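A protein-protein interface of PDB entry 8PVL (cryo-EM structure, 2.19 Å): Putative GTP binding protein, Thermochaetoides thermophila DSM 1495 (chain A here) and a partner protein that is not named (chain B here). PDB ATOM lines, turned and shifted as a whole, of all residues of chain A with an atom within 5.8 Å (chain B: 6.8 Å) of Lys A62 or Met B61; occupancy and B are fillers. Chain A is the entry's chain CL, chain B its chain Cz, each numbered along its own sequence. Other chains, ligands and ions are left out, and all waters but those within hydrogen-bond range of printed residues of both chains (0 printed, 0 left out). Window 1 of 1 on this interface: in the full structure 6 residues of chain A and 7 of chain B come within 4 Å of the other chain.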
ATOM      1  N   ILE A  55      16.405  -5.673 -15.607  1.00  0.00           N
ATOM      2  CA  ILE A  55      15.317  -4.760 -15.261  1.00  0.00           C
ATOM      3  C   ILE A  55      15.566  -4.246 -13.847  1.00  0.00           C
ATOM      4  O   ILE A  55      15.880  -5.051 -12.960  1.00  0.00           O
ATOM      5  CB  ILE A  55      13.948  -5.457 -15.357  1.00  0.00           C
ATOM      6  CG1 ILE A  55      13.828  -6.212 -16.683  1.00  0.00           C
ATOM      7  CG2 ILE A  55      12.811  -4.460 -15.207  1.00  0.00           C
ATOM      8  CD1 ILE A  55      12.671  -7.181 -16.730  1.00  0.00           C
ATOM      9  N   PRO A  56      15.471  -2.936 -13.603  1.00  0.00           N
ATOM     10  CA  PRO A  56      15.671  -2.422 -12.243  1.00  0.00           C
ATOM     11  C   PRO A  56      14.586  -2.902 -11.294  1.00  0.00           C
ATOM     12  O   PRO A  56      13.428  -3.082 -11.677  1.00  0.00           O
ATOM     13  CB  PRO A  56      15.619  -0.900 -12.422  1.00  0.00           C
ATOM     14  CG  PRO A  56      15.849  -0.667 -13.872  1.00  0.00           C
ATOM     15  CD  PRO A  56      15.269  -1.848 -14.572  1.00  0.00           C
ATOM     16  N   ASN A  57      14.979  -3.102 -10.035  1.00  0.00           N
ATOM     17  CA  ASN A  57      14.048  -3.618  -9.038  1.00  0.00           C
ATOM     18  C   ASN A  57      12.992  -2.589  -8.660  1.00  0.00           C
ATOM     19  O   ASN A  57      11.861  -2.957  -8.326  1.00  0.00           O
ATOM     20  CB  ASN A  57      14.814  -4.070  -7.795  1.00  0.00           C
ATOM     21  CG  ASN A  57      15.678  -5.285  -8.057  1.00  0.00           C
ATOM     22  OD1 ASN A  57      15.365  -6.111  -8.913  1.00  0.00           O
ATOM     23  ND2 ASN A  57      16.775  -5.400  -7.321  1.00  0.00           N
ATOM     24  N   PHE A  59      11.454  -0.491 -10.539  1.00  0.00           N
ATOM     25  CA  PHE A  59      10.406  -0.347 -11.538  1.00  0.00           C
ATOM     26  C   PHE A  59       9.159  -1.081 -11.057  1.00  0.00           C
ATOM     27  O   PHE A  59       9.217  -2.299 -10.831  1.00  0.00           O
ATOM     28  CB  PHE A  59      10.880  -0.898 -12.880  1.00  0.00           C
ATOM     29  CG  PHE A  59       9.863  -0.791 -13.979  1.00  0.00           C
ATOM     30  CD1 PHE A  59       9.386   0.445 -14.383  1.00  0.00           C
ATOM     31  CD2 PHE A  59       9.395  -1.927 -14.617  1.00  0.00           C
ATOM     32  CE1 PHE A  59       8.453   0.544 -15.397  1.00  0.00           C
ATOM     33  CE2 PHE A  59       8.463  -1.834 -15.633  1.00  0.00           C
ATOM     34  CZ  PHE A  59       7.991  -0.597 -16.023  1.00  0.00           C
ATOM     35  N   PRO A  60       8.026  -0.393 -10.885  1.00  0.00           N
ATOM     36  CA  PRO A  60       6.890  -1.006 -10.174  1.00  0.00           C
ATOM     37  C   PRO A  60       6.183  -2.106 -10.945  1.00  0.00           C
ATOM     38  O   PRO A  60       5.441  -2.882 -10.331  1.00  0.00           O
ATOM     39  CB  PRO A  60       5.950   0.183  -9.920  1.00  0.00           C
ATOM     40  CG  PRO A  60       6.782   1.411 -10.168  1.00  0.00           C
ATOM     41  CD  PRO A  60       7.769   1.018 -11.211  1.00  0.00           C
ATOM     42  N   TYR A  61       6.380  -2.207 -12.257  1.00  0.00           N
ATOM     43  CA  TYR A  61       5.721  -3.221 -13.070  1.00  0.00           C
ATOM     44  C   TYR A  61       6.712  -4.256 -13.596  1.00  0.00           C
ATOM     45  O   TYR A  61       6.514  -4.831 -14.671  1.00  0.00           O
ATOM     46  CB  TYR A  61       4.951  -2.561 -14.212  1.00  0.00           C
ATOM     47  CG  TYR A  61       4.022  -1.467 -13.736  1.00  0.00           C
ATOM     48  CD1 TYR A  61       3.170  -1.677 -12.658  1.00  0.00           C
ATOM     49  CD2 TYR A  61       4.010  -0.221 -14.347  1.00  0.00           C
ATOM     50  CE1 TYR A  61       2.323  -0.682 -12.212  1.00  0.00           C
ATOM     51  CE2 TYR A  61       3.165   0.782 -13.907  1.00  0.00           C
ATOM     52  CZ  TYR A  61       2.326   0.546 -12.839  1.00  0.00           C
ATOM     53  OH  TYR A  61       1.484   1.538 -12.396  1.00  0.00           O
ATOM     54  N   LYS A  62       7.780  -4.501 -12.830  1.00  0.00           N
ATOM     55  CA  LYS A  62       8.777  -5.494 -13.216  1.00  0.00           C
ATOM     56  C   LYS A  62       8.187  -6.899 -13.220  1.00  0.00           C
ATOM     57  O   LYS A  62       8.507  -7.708 -14.099  1.00  0.00           O
ATOM     58  CB  LYS A  62       9.983  -5.414 -12.276  1.00  0.00           C
ATOM     59  CG  LYS A  62      11.041  -6.476 -12.523  1.00  0.00           C
ATOM     60  CD  LYS A  62      12.335  -6.172 -11.795  1.00  0.00           C
ATOM     61  CE  LYS A  62      13.374  -7.247 -12.067  1.00  0.00           C
ATOM     62  NZ  LYS A  62      14.677  -6.953 -11.418  1.00  0.00           N
ATOM     63  N   GLU A  63       7.324  -7.207 -12.249  1.00  0.00           N
ATOM     64  CA  GLU A  63       6.687  -8.521 -12.208  1.00  0.00           C
ATOM     65  C   GLU A  63       5.766  -8.733 -13.404  1.00  0.00           C
ATOM     66  O   GLU A  63       5.729  -9.827 -13.981  1.00  0.00           O
ATOM     67  CB  GLU A  63       5.917  -8.689 -10.898  1.00  0.00           C
ATOM     68  CG  GLU A  63       5.320 -10.071 -10.700  1.00  0.00           C
ATOM     69  CD  GLU A  63       5.367 -10.525  -9.255  1.00  0.00           C
ATOM     70  OE1 GLU A  63       5.303  -9.661  -8.355  1.00  0.00           O
ATOM     71  OE2 GLU A  63       5.468 -11.747  -9.016  1.00  0.00           O
ATOM     72  N   ARG A  64       5.026  -7.695 -13.801  1.00  0.00           N
ATOM     73  CA  ARG A  64       4.180  -7.797 -14.986  1.00  0.00           C
ATOM     74  C   ARG A  64       5.016  -7.929 -16.254  1.00  0.00           C
ATOM     75  O   ARG A  64       4.629  -8.642 -17.188  1.00  0.00           O
ATOM     76  CB  ARG A  64       3.250  -6.589 -15.069  1.00  0.00           C
ATOM     77  CG  ARG A  64       2.520  -6.297 -13.771  1.00  0.00           C
ATOM     78  CD  ARG A  64       1.228  -5.534 -14.005  1.00  0.00           C
ATOM     79  NE  ARG A  64       1.366  -4.519 -15.041  1.00  0.00           N
ATOM     80  CZ  ARG A  64       0.855  -3.299 -14.963  1.00  0.00           C
ATOM     81  NH1 ARG A  64       0.166  -2.904 -13.905  1.00  0.00           N
ATOM     82  NH2 ARG A  64       1.040  -2.453 -15.973  1.00  0.00           N
ATOM     83  N   LEU A  65       6.170  -7.255 -16.302  1.00  0.00           N
ATOM     84  CA  LEU A  65       7.073  -7.421 -17.436  1.00  0.00           C
ATOM     85  C   LEU A  65       7.628  -8.841 -17.505  1.00  0.00           C
ATOM     86  O   LEU A  65       7.751  -9.413 -18.594  1.00  0.00           O
ATOM     87  CB  LEU A  65       8.208  -6.401 -17.358  1.00  0.00           C
ATOM     88  CG  LEU A  65       9.134  -6.305 -18.570  1.00  0.00           C
ATOM     89  CD1 LEU A  65       8.338  -6.236 -19.864  1.00  0.00           C
ATOM     90  CD2 LEU A  65      10.045  -5.097 -18.441  1.00  0.00           C
ATOM     91  N   LEU A  66       7.962  -9.425 -16.349  1.00  0.00           N
ATOM     92  CA  LEU A  66       8.420 -10.811 -16.313  1.00  0.00           C
ATOM     93  C   LEU A  66       7.320 -11.768 -16.756  1.00  0.00           C
ATOM     94  O   LEU A  66       7.585 -12.747 -17.468  1.00  0.00           O
ATOM     95  CB  LEU A  66       8.905 -11.167 -14.906  1.00  0.00           C
ATOM     96  CG  LEU A  66      10.188 -10.497 -14.411  1.00  0.00           C
ATOM     97  CD1 LEU A  66      10.419 -10.804 -12.942  1.00  0.00           C
ATOM     98  CD2 LEU A  66      11.381 -10.929 -15.243  1.00  0.00           C
ATOM     99  N   GLN A  67       6.076 -11.494 -16.347  1.00  0.00           N
ATOM    100  CA  GLN A  67       4.935 -12.275 -16.819  1.00  0.00           C
ATOM    101  C   GLN A  67       4.796 -12.195 -18.334  1.00  0.00           C
ATOM    102  O   GLN A  67       4.576 -13.215 -18.997  1.00  0.00           O
ATOM    103  CB  GLN A  67       3.648 -11.787 -16.153  1.00  0.00           C
ATOM    104  CG  GLN A  67       3.223 -12.575 -14.933  1.00  0.00           C
ATOM    105  CD  GLN A  67       2.736 -11.689 -13.806  1.00  0.00           C
ATOM    106  OE1 GLN A  67       2.010 -10.721 -14.034  1.00  0.00           O
ATOM    107  NE2 GLN A  67       3.131 -12.015 -12.582  1.00  0.00           N
ATOM    108  N   GLN B  56       6.351  -7.739   0.722  1.00  0.00           N
ATOM    109  CA  GLN B  56       5.926  -9.060   0.251  1.00  0.00           C
ATOM    110  C   GLN B  56       5.949  -9.147  -1.272  1.00  0.00           C
ATOM    111  O   GLN B  56       6.413 -10.150  -1.839  1.00  0.00           O
ATOM    112  CB  GLN B  56       4.534  -9.401   0.782  1.00  0.00           C
ATOM    113  CG  GLN B  56       4.344  -9.146   2.263  1.00  0.00           C
ATOM    114  CD  GLN B  56       2.903  -9.306   2.703  1.00  0.00           C
ATOM    115  OE1 GLN B  56       2.034  -9.661   1.907  1.00  0.00           O
ATOM    116  NE2 GLN B  56       2.642  -9.050   3.980  1.00  0.00           N
ATOM    117  N   GLU B  57       5.469  -8.100  -1.952  1.00  0.00           N
ATOM    118  CA  GLU B  57       5.461  -8.107  -3.414  1.00  0.00           C
ATOM    119  C   GLU B  57       6.877  -8.117  -3.987  1.00  0.00           C
ATOM    120  O   GLU B  57       7.151  -8.830  -4.962  1.00  0.00           O
ATOM    121  CB  GLU B  57       4.670  -6.911  -3.936  1.00  0.00           C
ATOM    122  CG  GLU B  57       3.177  -7.021  -3.685  1.00  0.00           C
ATOM    123  CD  GLU B  57       2.443  -5.721  -3.926  1.00  0.00           C
ATOM    124  OE1 GLU B  57       3.111  -4.687  -4.135  1.00  0.00           O
ATOM    125  OE2 GLU B  57       1.196  -5.732  -3.911  1.00  0.00           O
ATOM    126  N   GLN B  58       7.789  -7.347  -3.387  1.00  0.00           N
ATOM    127  CA  GLN B  58       9.173  -7.326  -3.848  1.00  0.00           C
ATOM    128  C   GLN B  58       9.858  -8.667  -3.621  1.00  0.00           C
ATOM    129  O   GLN B  58      10.641  -9.117  -4.466  1.00  0.00           O
ATOM    130  CB  GLN B  58       9.944  -6.206  -3.150  1.00  0.00           C
ATOM    131  CG  GLN B  58      11.186  -5.745  -3.896  1.00  0.00           C
ATOM    132  CD  GLN B  58      10.888  -4.673  -4.927  1.00  0.00           C
ATOM    133  OE1 GLN B  58       9.731  -4.347  -5.187  1.00  0.00           O
ATOM    134  NE2 GLN B  58      11.938  -4.118  -5.523  1.00  0.00           N
ATOM    135  N   ALA B  59       9.579  -9.318  -2.485  1.00  0.00           N
ATOM    136  CA  ALA B  59      10.151 -10.637  -2.229  1.00  0.00           C
ATOM    137  C   ALA B  59       9.660 -11.666  -3.241  1.00  0.00           C
ATOM    138  O   ALA B  59      10.451 -12.477  -3.748  1.00  0.00           O
ATOM    139  CB  ALA B  59       9.820 -11.081  -0.804  1.00  0.00           C
ATOM    140  N   ALA B  60       8.360 -11.637  -3.561  1.00  0.00           N
ATOM    141  CA  ALA B  60       7.822 -12.556  -4.564  1.00  0.00           C
ATOM    142  C   ALA B  60       8.432 -12.302  -5.942  1.00  0.00           C
ATOM    143  O   ALA B  60       8.773 -13.252  -6.666  1.00  0.00           O
ATOM    144  CB  ALA B  60       6.300 -12.435  -4.618  1.00  0.00           C
ATOM    145  N   MET B  61       8.592 -11.027  -6.312  1.00  0.00           N
ATOM    146  CA  MET B  61       9.212 -10.686  -7.591  1.00  0.00           C
ATOM    147  C   MET B  61      10.659 -11.166  -7.657  1.00  0.00           C
ATOM    148  O   MET B  61      11.099 -11.694  -8.689  1.00  0.00           O
ATOM    149  CB  MET B  61       9.109  -9.173  -7.821  1.00  0.00           C
ATOM    150  CG  MET B  61       9.788  -8.614  -9.081  1.00  0.00           C
ATOM    151  SD  MET B  61      11.575  -8.314  -9.018  1.00  0.00           S
ATOM    152  CE  MET B  61      11.664  -6.926  -7.891  1.00  0.00           C
ATOM    153  N   LYS B  62      11.419 -10.973  -6.572  1.00  0.00           N
ATOM    154  CA  LYS B  62      12.814 -11.406  -6.552  1.00  0.00           C
ATOM    155  C   LYS B  62      12.923 -12.924  -6.646  1.00  0.00           C
ATOM    156  O   LYS B  62      13.825 -13.445  -7.317  1.00  0.00           O
ATOM    157  CB  LYS B  62      13.514 -10.888  -5.294  1.00  0.00           C
ATOM    158  CG  LYS B  62      13.792  -9.386  -5.293  1.00  0.00           C
ATOM    159  CD  LYS B  62      15.240  -9.089  -5.654  1.00  0.00           C
ATOM    160  CE  LYS B  62      15.407  -8.912  -7.153  1.00  0.00           C
ATOM    161  NZ  LYS B  62      16.801  -8.587  -7.546  1.00  0.00           N
ATOM    162  N   ALA B  63      12.003 -13.643  -5.995  1.00  0.00           N
ATOM    163  CA  ALA B  63      11.970 -15.100  -6.110  1.00  0.00           C
ATOM    164  C   ALA B  63      11.715 -15.543  -7.547  1.00  0.00           C
ATOM    165  O   ALA B  63      12.398 -16.438  -8.066  1.00  0.00           O
ATOM    166  CB  ALA B  63      10.900 -15.667  -5.177  1.00  0.00           C
ATOM    167  N   LYS B  64      10.741 -14.914  -8.213  1.00  0.00           N
ATOM    168  CA  LYS B  64      10.429 -15.293  -9.590  1.00  0.00           C
ATOM    169  C   LYS B  64      11.600 -15.010 -10.529  1.00  0.00           C
ATOM    170  O   LYS B  64      11.918 -15.824 -11.412  1.00  0.00           O
ATOM    171  CB  LYS B  64       9.173 -14.565 -10.060  1.00  0.00           C
ATOM    172  CG  LYS B  64       8.807 -14.885 -11.489  1.00  0.00           C
ATOM    173  CD  LYS B  64       7.548 -14.187 -11.948  1.00  0.00           C
ATOM    174  CE  LYS B  64       7.194 -14.639 -13.357  1.00  0.00           C
ATOM    175  NZ  LYS B  64       5.890 -14.112 -13.805  1.00  0.00           N
ATOM    176  N   GLU B  65      12.266 -13.868 -10.338  1.00  0.00           N
ATOM    177  CA  GLU B  65      13.429 -13.547 -11.161  1.00  0.00           C
ATOM    178  C   GLU B  65      14.571 -14.527 -10.911  1.00  0.00           C
ATOM    179  O   GLU B  65      15.285 -14.907 -11.850  1.00  0.00           O
ATOM    180  CB  GLU B  65      13.873 -12.108 -10.895  1.00  0.00           C
ATOM    181  CG  GLU B  65      14.967 -11.619 -11.827  1.00  0.00           C
ATOM    182  CD  GLU B  65      15.523 -10.271 -11.421  1.00  0.00           C
ATOM    183  OE1 GLU B  65      15.186  -9.795 -10.317  1.00  0.00           O
ATOM    184  OE2 GLU B  65      16.304  -9.690 -12.202  1.00  0.00           O
ATOM    185  N   ARG B  66      14.745 -14.959  -9.657  1.00  0.00           N
ATOM    186  CA  ARG B  66      15.797 -15.919  -9.333  1.00  0.00           C
ATOM    187  C   ARG B  66      15.558 -17.261 -10.018  1.00  0.00           C
ATOM    188  O   ARG B  66      16.482 -17.840 -10.604  1.00  0.00           O
ATOM    189  CB  ARG B  66      15.893 -16.097  -7.819  1.00  0.00           C
ATOM    190  CG  ARG B  66      17.274 -15.824  -7.251  1.00  0.00           C
ATOM    191  CD  ARG B  66      17.336 -16.157  -5.770  1.00  0.00           C
ATOM    192  NE  ARG B  66      16.142 -15.714  -5.063  1.00  0.00           N
ATOM    193  CZ  ARG B  66      16.051 -14.571  -4.397  1.00  0.00           C
ATOM    194  NH1 ARG B  66      17.070 -13.731  -4.325  1.00  0.00           N
ATOM    195  NH2 ARG B  66      14.909 -14.264  -3.789  1.00  0.00           N
ATOM    196  N   LYS B  69      16.242 -16.821 -13.857  1.00  0.00           N
ATOM    197  CA  LYS B  69      17.677 -16.796 -14.127  1.00  0.00           C
ATOM    198  C   LYS B  69      18.303 -18.175 -13.958  1.00  0.00           C
ATOM    199  O   LYS B  69      19.193 -18.553 -14.730  1.00  0.00           O
ATOM    200  CB  LYS B  69      18.363 -15.787 -13.208  1.00  0.00           C
ATOM    201  CG  LYS B  69      18.163 -14.336 -13.606  1.00  0.00           C
ATOM    202  CD  LYS B  69      18.810 -13.406 -12.594  1.00  0.00           C
ATOM    203  CE  LYS B  69      18.792 -11.965 -13.069  1.00  0.00           C
ATOM    204  NZ  LYS B  69      19.337 -11.038 -12.038  1.00  0.00           N
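Among the printed residues, pairs that only touch across the chains: Gln A67 with Lys B64 (3.3 Å), Lys A62 with Met B61 (3.6 Å), Glu A63 with Met B61 (3.9 Å), Asn A57 with Met B61 (3.9 Å), Asn A57 with Glu B65 (3.9 Å) and Glu A63 with Glu B57 (3.95 Å).
Printed residues of chain A that touch a printed residue of chain B: Asn A57, Lys A62, Glu A63 and Gln A67.
Printed residues of chain B within 4 Å of Asn A57: Gln B58, Met B61, Lys B62 and Glu B65. Lys A62 touches just these residues of chain B: Met B61 (3.6 Å) and Glu B65 (3.1 Å). Printed residues of chain B within 4 Å of Glu A63: Glu B57 (3.95 Å) and Met B61 (3.9 Å). Of the printed residues of chain B, Gln A67 touches Lys B64. Printed residues of chain A within 4 Å of Gln B58: Asn A57. Met B61 touches just these residues of chain A: Asn A57, Lys A62 and Glu A63. Printed residues of chain A within 4 Å of Lys B64: Gln A67 (3.3 Å). The nearest residue of chain B that does not touch Lys A62 is Lys B62 (4.7 Å). The nearest residue of chain A that does not touch Met B61 is Leu A66 (4.4 Å).
The side-chain amide oxygen (OD1) of Asn A57 sits at hydrogen-bond distance from the side-chain amino group (NZ) of Lys A62. NZ of Lys B69 lies within salt-bridge range of OE2 of Glu B65, at 3.3 Å. NZ of Lys A62 lies within hydrogen-bond range of O of Ile A55 (2.7 Å). NZ of Lys B62 lies within salt-bridge range of OE1 of Glu B65.
NZ of Lys A62 lies within salt-bridge range of OE1 of Glu B65. The side-chain amide oxygen of Asn A57 is in hydrogen-bond range of the side-chain amino group of Lys B62. The side-chain amide nitrogen (NE2) of Gln B58 sits at hydrogen-bond distance from the backbone carbonyl oxygen (O) of Asn A57.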
